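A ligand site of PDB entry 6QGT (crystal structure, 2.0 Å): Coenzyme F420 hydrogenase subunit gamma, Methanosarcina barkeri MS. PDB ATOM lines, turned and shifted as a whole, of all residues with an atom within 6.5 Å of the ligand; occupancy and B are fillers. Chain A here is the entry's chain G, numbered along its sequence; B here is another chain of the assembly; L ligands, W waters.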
ATOM      1  N   HIS A  10      13.728   2.196  12.570  1.00  0.00           N
ATOM      2  CA  HIS A  10      14.590   1.068  12.868  1.00  0.00           C
ATOM      3  C   HIS A  10      13.722  -0.102  13.293  1.00  0.00           C
ATOM      4  O   HIS A  10      13.244  -0.143  14.418  1.00  0.00           O
ATOM      5  CB  HIS A  10      15.582   1.421  13.960  1.00  0.00           C
ATOM      6  CG  HIS A  10      16.528   0.317  14.289  1.00  0.00           C
ATOM      7  ND1 HIS A  10      17.496  -0.115  13.417  1.00  0.00           N
ATOM      8  CD2 HIS A  10      16.627  -0.465  15.399  1.00  0.00           C
ATOM      9  CE1 HIS A  10      18.164  -1.124  13.970  1.00  0.00           C
ATOM     10  NE2 HIS A  10      17.645  -1.355  15.161  1.00  0.00           N
ATOM     11  N   SER A  12      13.825  -4.558  12.756  1.00  0.00           N
ATOM     12  CA  SER A  12      14.806  -5.551  13.201  1.00  0.00           C
ATOM     13  C   SER A  12      16.002  -5.457  12.261  1.00  0.00           C
ATOM     14  O   SER A  12      16.173  -6.257  11.324  1.00  0.00           O
ATOM     15  CB  SER A  12      14.201  -6.944  13.241  1.00  0.00           C
ATOM     16  OG  SER A  12      13.513  -7.147  14.474  1.00  0.00           O
ATOM     17  N   GLY A  13      16.814  -4.418  12.471  1.00  0.00           N
ATOM     18  CA  GLY A  13      17.954  -4.114  11.642  1.00  0.00           C
ATOM     19  C   GLY A  13      19.203  -4.036  12.508  1.00  0.00           C
ATOM     20  O   GLY A  13      19.152  -4.252  13.715  1.00  0.00           O
ATOM     21  N   CYS A  14      20.338  -3.745  11.859  1.00  0.00           N
ATOM     22  CA  CYS A  14      21.604  -3.711  12.594  1.00  0.00           C
ATOM     23  C   CYS A  14      22.136  -2.285  12.783  1.00  0.00           C
ATOM     24  O   CYS A  14      23.189  -2.107  13.432  1.00  0.00           O
ATOM     25  CB  CYS A  14      22.660  -4.572  11.876  1.00  0.00           C
ATOM     26  SG  CYS A  14      23.492  -3.754  10.539  1.00  0.00           S
ATOM     27  N   THR A  15      21.456  -1.281  12.226  1.00  0.00           N
ATOM     28  CA  THR A  15      21.760   0.143  12.232  1.00  0.00           C
ATOM     29  C   THR A  15      22.871   0.428  11.242  1.00  0.00           C
ATOM     30  O   THR A  15      23.204   1.594  11.021  1.00  0.00           O
ATOM     31  CB  THR A  15      22.096   0.652  13.648  1.00  0.00           C
ATOM     32  OG1 THR A  15      21.045   0.234  14.525  1.00  0.00           O
ATOM     33  CG2 THR A  15      22.200   2.181  13.725  1.00  0.00           C
ATOM     34  N   GLY A  16      23.423  -0.598  10.585  1.00  0.00           N
ATOM     35  CA  GLY A  16      24.395  -0.361   9.523  1.00  0.00           C
ATOM     36  C   GLY A  16      23.813   0.408   8.347  1.00  0.00           C
ATOM     37  O   GLY A  16      24.548   1.135   7.651  1.00  0.00           O
ATOM     38  N   CYS A  17      22.507   0.288   8.114  1.00  0.00           N
ATOM     39  CA  CYS A  17      21.866   1.125   7.117  1.00  0.00           C
ATOM     40  C   CYS A  17      21.924   2.606   7.520  1.00  0.00           C
ATOM     41  O   CYS A  17      22.221   3.466   6.685  1.00  0.00           O
ATOM     42  CB  CYS A  17      20.427   0.665   6.897  1.00  0.00           C
ATOM     43  SG  CYS A  17      20.387  -0.807   5.826  1.00  0.00           S
ATOM     44  N   LEU A  18      21.672   2.929   8.794  1.00  0.00           N
ATOM     45  CA  LEU A  18      21.834   4.313   9.229  1.00  0.00           C
ATOM     46  C   LEU A  18      23.282   4.762   9.111  1.00  0.00           C
ATOM     47  O   LEU A  18      23.552   5.880   8.653  1.00  0.00           O
ATOM     48  CB  LEU A  18      21.325   4.488  10.657  1.00  0.00           C
ATOM     49  CG  LEU A  18      21.419   5.954  11.128  1.00  0.00           C
ATOM     50  CD1 LEU A  18      20.593   6.893  10.250  1.00  0.00           C
ATOM     51  CD2 LEU A  18      20.980   6.085  12.562  1.00  0.00           C
ATOM     52  N   SER A  20      25.425   3.788   7.000  1.00  0.00           N
ATOM     53  CA  SER A  20      25.677   4.051   5.590  1.00  0.00           C
ATOM     54  C   SER A  20      25.172   5.441   5.184  1.00  0.00           C
ATOM     55  O   SER A  20      25.837   6.134   4.408  1.00  0.00           O
ATOM     56  CB  SER A  20      25.031   2.973   4.727  1.00  0.00           C
ATOM     57  OG  SER A  20      25.574   1.716   5.090  1.00  0.00           O
ATOM     58  N   GLU A  59      14.671   0.587   7.897  1.00  0.00           N
ATOM     59  CA  GLU A  59      15.649  -0.484   7.884  1.00  0.00           C
ATOM     60  C   GLU A  59      15.178  -1.665   8.737  1.00  0.00           C
ATOM     61  O   GLU A  59      14.365  -1.522   9.655  1.00  0.00           O
ATOM     62  CB  GLU A  59      17.010   0.007   8.373  1.00  0.00           C
ATOM     63  CG  GLU A  59      17.093   0.213   9.853  1.00  0.00           C
ATOM     64  CD  GLU A  59      18.550   0.278  10.295  1.00  0.00           C
ATOM     65  OE1 GLU A  59      19.223   1.296  10.015  1.00  0.00           O
ATOM     66  OE2 GLU A  59      19.035  -0.713  10.852  1.00  0.00           O
ATOM     67  N   GLY A  60      15.709  -2.851   8.409  1.00  0.00           N
ATOM     68  CA  GLY A  60      15.403  -4.049   9.155  1.00  0.00           C
ATOM     69  C   GLY A  60      14.060  -4.662   8.762  1.00  0.00           C
ATOM     70  O   GLY A  60      13.226  -4.038   8.095  1.00  0.00           O
ATOM     71  N   LEU A  86      14.914   0.601   3.281  1.00  0.00           N
ATOM     72  CA  LEU A  86      16.341   0.933   3.276  1.00  0.00           C
ATOM     73  C   LEU A  86      17.141  -0.309   3.640  1.00  0.00           C
ATOM     74  O   LEU A  86      17.020  -0.814   4.765  1.00  0.00           O
ATOM     75  CB  LEU A  86      16.648   2.046   4.288  1.00  0.00           C
ATOM     76  CG  LEU A  86      18.142   2.344   4.459  1.00  0.00           C
ATOM     77  CD1 LEU A  86      18.813   2.697   3.162  1.00  0.00           C
ATOM     78  CD2 LEU A  86      18.326   3.447   5.468  1.00  0.00           C
ATOM     79  N   GLY A  87      17.954  -0.794   2.701  1.00  0.00           N
ATOM     80  CA  GLY A  87      18.796  -1.959   2.939  1.00  0.00           C
ATOM     81  C   GLY A  87      18.084  -3.293   2.754  1.00  0.00           C
ATOM     82  O   GLY A  87      16.854  -3.384   2.698  1.00  0.00           O
ATOM     83  N   SER A  88      18.897  -4.361   2.710  1.00  0.00           N
ATOM     84  CA  SER A  88      18.417  -5.678   2.292  1.00  0.00           C
ATOM     85  C   SER A  88      17.514  -6.354   3.330  1.00  0.00           C
ATOM     86  O   SER A  88      16.646  -7.153   2.941  1.00  0.00           O
ATOM     87  CB  SER A  88      19.605  -6.589   1.958  1.00  0.00           C
ATOM     88  OG  SER A  88      20.274  -6.091   0.826  1.00  0.00           O
ATOM     89  N   CYS A  89      17.692  -6.078   4.630  1.00  0.00           N
ATOM     90  CA  CYS A  89      16.765  -6.645   5.602  1.00  0.00           C
ATOM     91  C   CYS A  89      15.360  -6.130   5.363  1.00  0.00           C
ATOM     92  O   CYS A  89      14.390  -6.910   5.406  1.00  0.00           O
ATOM     93  CB  CYS A  89      17.168  -6.269   7.037  1.00  0.00           C
ATOM     94  SG  CYS A  89      18.725  -6.982   7.628  1.00  0.00           S
ATOM     95  N   ALA A  90      15.230  -4.808   5.155  1.00  0.00           N
ATOM     96  CA  ALA A  90      13.909  -4.240   4.894  1.00  0.00           C
ATOM     97  C   ALA A  90      13.348  -4.721   3.541  1.00  0.00           C
ATOM     98  O   ALA A  90      12.161  -5.082   3.445  1.00  0.00           O
ATOM     99  CB  ALA A  90      13.973  -2.716   4.977  1.00  0.00           C
ATOM    100  N   GLY A  93      14.489  -9.350   3.745  1.00  0.00           N
ATOM    101  CA  GLY A  93      14.693 -10.219   4.898  1.00  0.00           C
ATOM    102  C   GLY A  93      16.151 -10.444   5.264  1.00  0.00           C
ATOM    103  O   GLY A  93      16.502 -10.341   6.442  1.00  0.00           O
ATOM    104  N   ASN A  94      16.993 -10.746   4.277  1.00  0.00           N
ATOM    105  CA  ASN A  94      18.468 -10.819   4.463  1.00  0.00           C
ATOM    106  C   ASN A  94      18.754 -11.861   5.546  1.00  0.00           C
ATOM    107  O   ASN A  94      18.150 -12.956   5.523  1.00  0.00           O
ATOM    108  CB  ASN A  94      18.967  -9.399   4.725  1.00  0.00           C
ATOM    109  CG  ASN A  94      20.506  -9.257   4.672  1.00  0.00           C
ATOM    110  OD1 ASN A  94      21.150  -9.530   3.652  1.00  0.00           O
ATOM    111  ND2 ASN A  94      21.068  -8.749   5.757  1.00  0.00           N
ATOM    112  N   ILE A  95      19.590 -11.569   6.560  1.00  0.00           N
ATOM    113  CA  ILE A  95      19.975 -12.624   7.498  1.00  0.00           C
ATOM    114  C   ILE A  95      18.804 -13.052   8.362  1.00  0.00           C
ATOM    115  O   ILE A  95      18.852 -14.147   8.950  1.00  0.00           O
ATOM    116  CB  ILE A  95      21.171 -12.215   8.387  1.00  0.00           C
ATOM    117  CG1 ILE A  95      20.833 -10.997   9.269  1.00  0.00           C
ATOM    118  CG2 ILE A  95      22.447 -11.953   7.493  1.00  0.00           C
ATOM    119  CD1 ILE A  95      21.477 -11.041  10.691  1.00  0.00           C
ATOM    120  N   GLY A 127      20.882  -3.739  -0.655  1.00  0.00           N
ATOM    121  CA  GLY A 127      22.288  -3.768  -0.325  1.00  0.00           C
ATOM    122  C   GLY A 127      22.481  -4.068   1.149  1.00  0.00           C
ATOM    123  O   GLY A 127      21.681  -3.666   2.010  1.00  0.00           O
ATOM    124  N   CYS A 128      23.539  -4.810   1.455  1.00  0.00           N
ATOM    125  CA  CYS A 128      23.916  -5.081   2.836  1.00  0.00           C
ATOM    126  C   CYS A 128      25.440  -5.113   2.890  1.00  0.00           C
ATOM    127  O   CYS A 128      26.060  -6.129   2.558  1.00  0.00           O
ATOM    128  CB  CYS A 128      23.314  -6.386   3.345  1.00  0.00           C
ATOM    129  SG  CYS A 128      23.851  -6.763   5.026  1.00  0.00           S
ATOM    130  N   PRO A 129      26.081  -3.985   3.258  1.00  0.00           N
ATOM    131  CA  PRO A 129      25.394  -2.724   3.568  1.00  0.00           C
ATOM    132  C   PRO A 129      24.957  -1.985   2.288  1.00  0.00           C
ATOM    133  O   PRO A 129      25.600  -2.142   1.242  1.00  0.00           O
ATOM    134  CB  PRO A 129      26.474  -1.927   4.294  1.00  0.00           C
ATOM    135  CG  PRO A 129      27.720  -2.320   3.494  1.00  0.00           C
ATOM    136  CD  PRO A 129      27.540  -3.790   3.173  1.00  0.00           C
ATOM    137  N   PRO A 130      23.902  -1.167   2.376  1.00  0.00           N
ATOM    138  CA  PRO A 130      23.543  -0.307   1.239  1.00  0.00           C
ATOM    139  C   PRO A 130      24.611   0.746   1.001  1.00  0.00           C
ATOM    140  O   PRO A 130      25.213   1.244   1.941  1.00  0.00           O
ATOM    141  CB  PRO A 130      22.220   0.326   1.703  1.00  0.00           C
ATOM    142  CG  PRO A 130      22.353   0.349   3.207  1.00  0.00           C
ATOM    143  CD  PRO A 130      23.038  -0.948   3.550  1.00  0.00           C
ATOM    144  N   ARG B  41      16.647 -11.923  17.052  1.00  0.00           N
ATOM    145  CA  ARG B  41      16.825 -12.552  15.749  1.00  0.00           C
ATOM    146  C   ARG B  41      17.399 -13.978  15.872  1.00  0.00           C
ATOM    147  O   ARG B  41      17.216 -14.796  14.962  1.00  0.00           O
ATOM    148  CB  ARG B  41      17.705 -11.646  14.887  1.00  0.00           C
ATOM    149  CG  ARG B  41      17.017 -10.308  14.574  1.00  0.00           C
ATOM    150  CD  ARG B  41      17.967  -9.254  14.002  1.00  0.00           C
ATOM    151  NE  ARG B  41      18.889  -8.725  15.019  1.00  0.00           N
ATOM    152  CZ  ARG B  41      20.037  -8.135  14.729  1.00  0.00           C
ATOM    153  NH1 ARG B  41      20.387  -7.992  13.456  1.00  0.00           N
ATOM    154  NH2 ARG B  41      20.845  -7.689  15.684  1.00  0.00           N
ATOM    155  N   SER B  60      28.219 -10.929  11.711  1.00  0.00           N
ATOM    156  CA  SER B  60      28.534  -9.542  11.401  1.00  0.00           C
ATOM    157  C   SER B  60      27.277  -8.696  11.401  1.00  0.00           C
ATOM    158  O   SER B  60      27.257  -7.587  11.937  1.00  0.00           O
ATOM    159  CB  SER B  60      29.206  -9.436  10.048  1.00  0.00           C
ATOM    160  OG  SER B  60      29.719  -8.142   9.902  1.00  0.00           O
ATOM    161  N   ARG B  61      26.213  -9.234  10.823  1.00  0.00           N
ATOM    162  CA  ARG B  61      24.973  -8.502  10.630  1.00  0.00           C
ATOM    163  C   ARG B  61      24.161  -8.410  11.903  1.00  0.00           C
ATOM    164  O   ARG B  61      23.013  -7.932  11.870  1.00  0.00           O
ATOM    165  CB  ARG B  61      24.219  -9.143   9.466  1.00  0.00           C
ATOM    166  CG  ARG B  61      24.795  -8.589   8.158  1.00  0.00           C
ATOM    167  CD  ARG B  61      25.219  -9.637   7.132  1.00  0.00           C
ATOM    168  NE  ARG B  61      25.728  -8.968   5.935  1.00  0.00           N
ATOM    169  CZ  ARG B  61      26.954  -9.105   5.430  1.00  0.00           C
ATOM    170  NH1 ARG B  61      27.800  -9.955   6.012  1.00  0.00           N
ATOM    171  NH2 ARG B  61      27.331  -8.423   4.342  1.00  0.00           N
ATOM    172  N   VAL B  62      24.751  -8.809  13.027  1.00  0.00           N
ATOM    173  CA  VAL B  62      24.180  -8.464  14.319  1.00  0.00           C
ATOM    174  C   VAL B  62      24.159  -6.946  14.487  1.00  0.00           C
ATOM    175  O   VAL B  62      23.183  -6.395  15.020  1.00  0.00           O
ATOM    176  CB  VAL B  62      24.968  -9.144  15.451  1.00  0.00           C
ATOM    177  CG1 VAL B  62      24.596  -8.520  16.788  1.00  0.00           C
ATOM    178  CG2 VAL B  62      24.682 -10.648  15.476  1.00  0.00           C
ATOM    179  N   CYS B  63      25.205  -6.260  14.006  1.00  0.00           N
ATOM    180  CA  CYS B  63      25.365  -4.828  14.267  1.00  0.00           C
ATOM    181  C   CYS B  63      26.243  -4.161  13.220  1.00  0.00           C
ATOM    182  O   CYS B  63      27.352  -4.632  12.938  1.00  0.00           O
ATOM    183  CB  CYS B  63      25.942  -4.574  15.676  1.00  0.00           C
ATOM    184  SG  CYS B  63      26.259  -2.807  15.890  1.00  0.00           S
ATOM    185  N   GLY B  64      25.768  -3.044  12.684  1.00  0.00           N
ATOM    186  CA  GLY B  64      26.509  -2.309  11.679  1.00  0.00           C
ATOM    187  C   GLY B  64      27.387  -1.189  12.190  1.00  0.00           C
ATOM    188  O   GLY B  64      28.084  -0.532  11.407  1.00  0.00           O
ATOM    189  N   ILE B 161      31.482  -1.625   6.630  1.00  0.00           N
ATOM    190  CA  ILE B 161      30.346  -2.233   7.321  1.00  0.00           C
ATOM    191  C   ILE B 161      30.202  -3.643   6.776  1.00  0.00           C
ATOM    192  O   ILE B 161      29.924  -3.835   5.596  1.00  0.00           O
ATOM    193  CB  ILE B 161      29.060  -1.399   7.107  1.00  0.00           C
ATOM    194  CG1 ILE B 161      29.355   0.072   7.440  1.00  0.00           C
ATOM    195  CG2 ILE B 161      27.954  -1.934   7.968  1.00  0.00           C
ATOM    196  CD1 ILE B 161      28.333   1.071   6.925  1.00  0.00           C
ATOM    197  N   HIS B 162      30.390  -4.656   7.660  1.00  0.00           N
ATOM    198  CA  HIS B 162      30.381  -6.081   7.327  1.00  0.00           C
ATOM    199  C   HIS B 162      31.608  -6.382   6.486  1.00  0.00           C
ATOM    200  O   HIS B 162      31.514  -6.677   5.282  1.00  0.00           O
ATOM    201  CB  HIS B 162      29.078  -6.480   6.632  1.00  0.00           C
ATOM    202  CG  HIS B 162      27.866  -6.030   7.390  1.00  0.00           C
ATOM    203  ND1 HIS B 162      27.742  -6.245   8.751  1.00  0.00           N
ATOM    204  CD2 HIS B 162      26.775  -5.330   7.019  1.00  0.00           C
ATOM    205  CE1 HIS B 162      26.592  -5.730   9.166  1.00  0.00           C
ATOM    206  NE2 HIS B 162      25.986  -5.171   8.138  1.00  0.00           N
HETATM  207 FE1  LIG L   1      22.272  -4.119   8.709  1.00  0.00          FE
HETATM  208 FE2  LIG L   1      20.128  -5.331   7.476  1.00  0.00          FE
HETATM  209 FE3  LIG L   1      22.624  -5.219   6.256  1.00  0.00          FE
HETATM  210 FE4  LIG L   1      21.168  -2.785   6.666  1.00  0.00          FE
HETATM  211  S1  LIG L   1      20.527  -4.506   5.311  1.00  0.00           S
HETATM  212  S2  LIG L   1      23.498  -3.225   7.048  1.00  0.00           S
HETATM  213  S3  LIG L   1      19.985  -3.322   8.717  1.00  0.00           S
HETATM  214  S4  LIG L   1      22.214  -6.384   8.277  1.00  0.00           S
HETATM  215  O   HOH W   1      17.580  -3.055   6.214  1.00  0.00           O
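NE2 of His 162 of chain B lies close to S2 of the ligand, at 3.3 Å. ND2 of Asn 94 lies close to S4 of the ligand. The side-chain sulfur (SG) of Cys 14 binds an iron atom (FE1) of the ligand, 2.2 Å away. The side-chain sulfur (SG) of Cys 128 binds an iron atom (FE3) of the ligand, at 2.3 Å. N of Cys 89 lies close to S1 of the ligand (3.3 Å). The side-chain sulfur of Cys 17 binds an iron atom (FE4) of the ligand, at 2.3 Å. S3 of the ligand sits close to N of Cys 14 (3.2 Å). The backbone NH (N) of Ser 88 sits close to a sulfur (S1) of the ligand (3.1 Å). The side-chain sulfur of Cys 89 is bound to an iron atom (FE2) of the ligand.
The backbone NH (N) of Cys 14 is in hydrogen-bond range of the side-chain carboxylate (OE2) of Glu 59 (3.5 Å). O of Cys 128 lies within hydrogen-bond range of NH2 of Arg 61 of chain B, 3.2 Å away. The side-chain carboxylate (OE1) of Glu 59 sits at hydrogen-bond distance from the backbone NH (N) of Leu 18. The side-chain sulfur (SG) of Cys 14 sits close to a ring nitrogen (NE2) of His 162 of chain B (3.7 Å). The side-chain sulfur (SG) of Cys 17 lies close to the backbone carbonyl oxygen (O) of Leu 86, at 3.5 Å. ND1 of His 10 lies within hydrogen-bond range of OE2 of Glu 59, at 3.1 Å. The side-chain carboxylate (OE2) of Glu 59 is in hydrogen-bond range of the backbone NH (N) of Thr 15 (2.8 Å). O of Arg 61 of chain B sits at hydrogen-bond distance from NH1 of Arg 41 of chain B.
The side-chain carboxylate of Glu 59 sits close to a sulfur (S3) of the ligand (3.5 Å). The backbone carbonyl oxygen (O) of Gly 127 lies close to a sulfur (S1) of the ligand (3.6 Å). Gly 13 touches the ligand (CA to S3, 3.6 Å). Gly 16 touches the ligand. Gly 87 touches the ligand (C to S1, 3.7 Å). Pro 129 touches the ligand (CA to S2, 3.99 Å). CG of Arg 61 of chain B touches S4 of the ligand, at 3.4 Å. Hydrophobic or aromatic side chains within 4 Å of the ligand: His 162 of chain B. Of the 31 residues printed, 14 come within 4 Å of the ligand.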
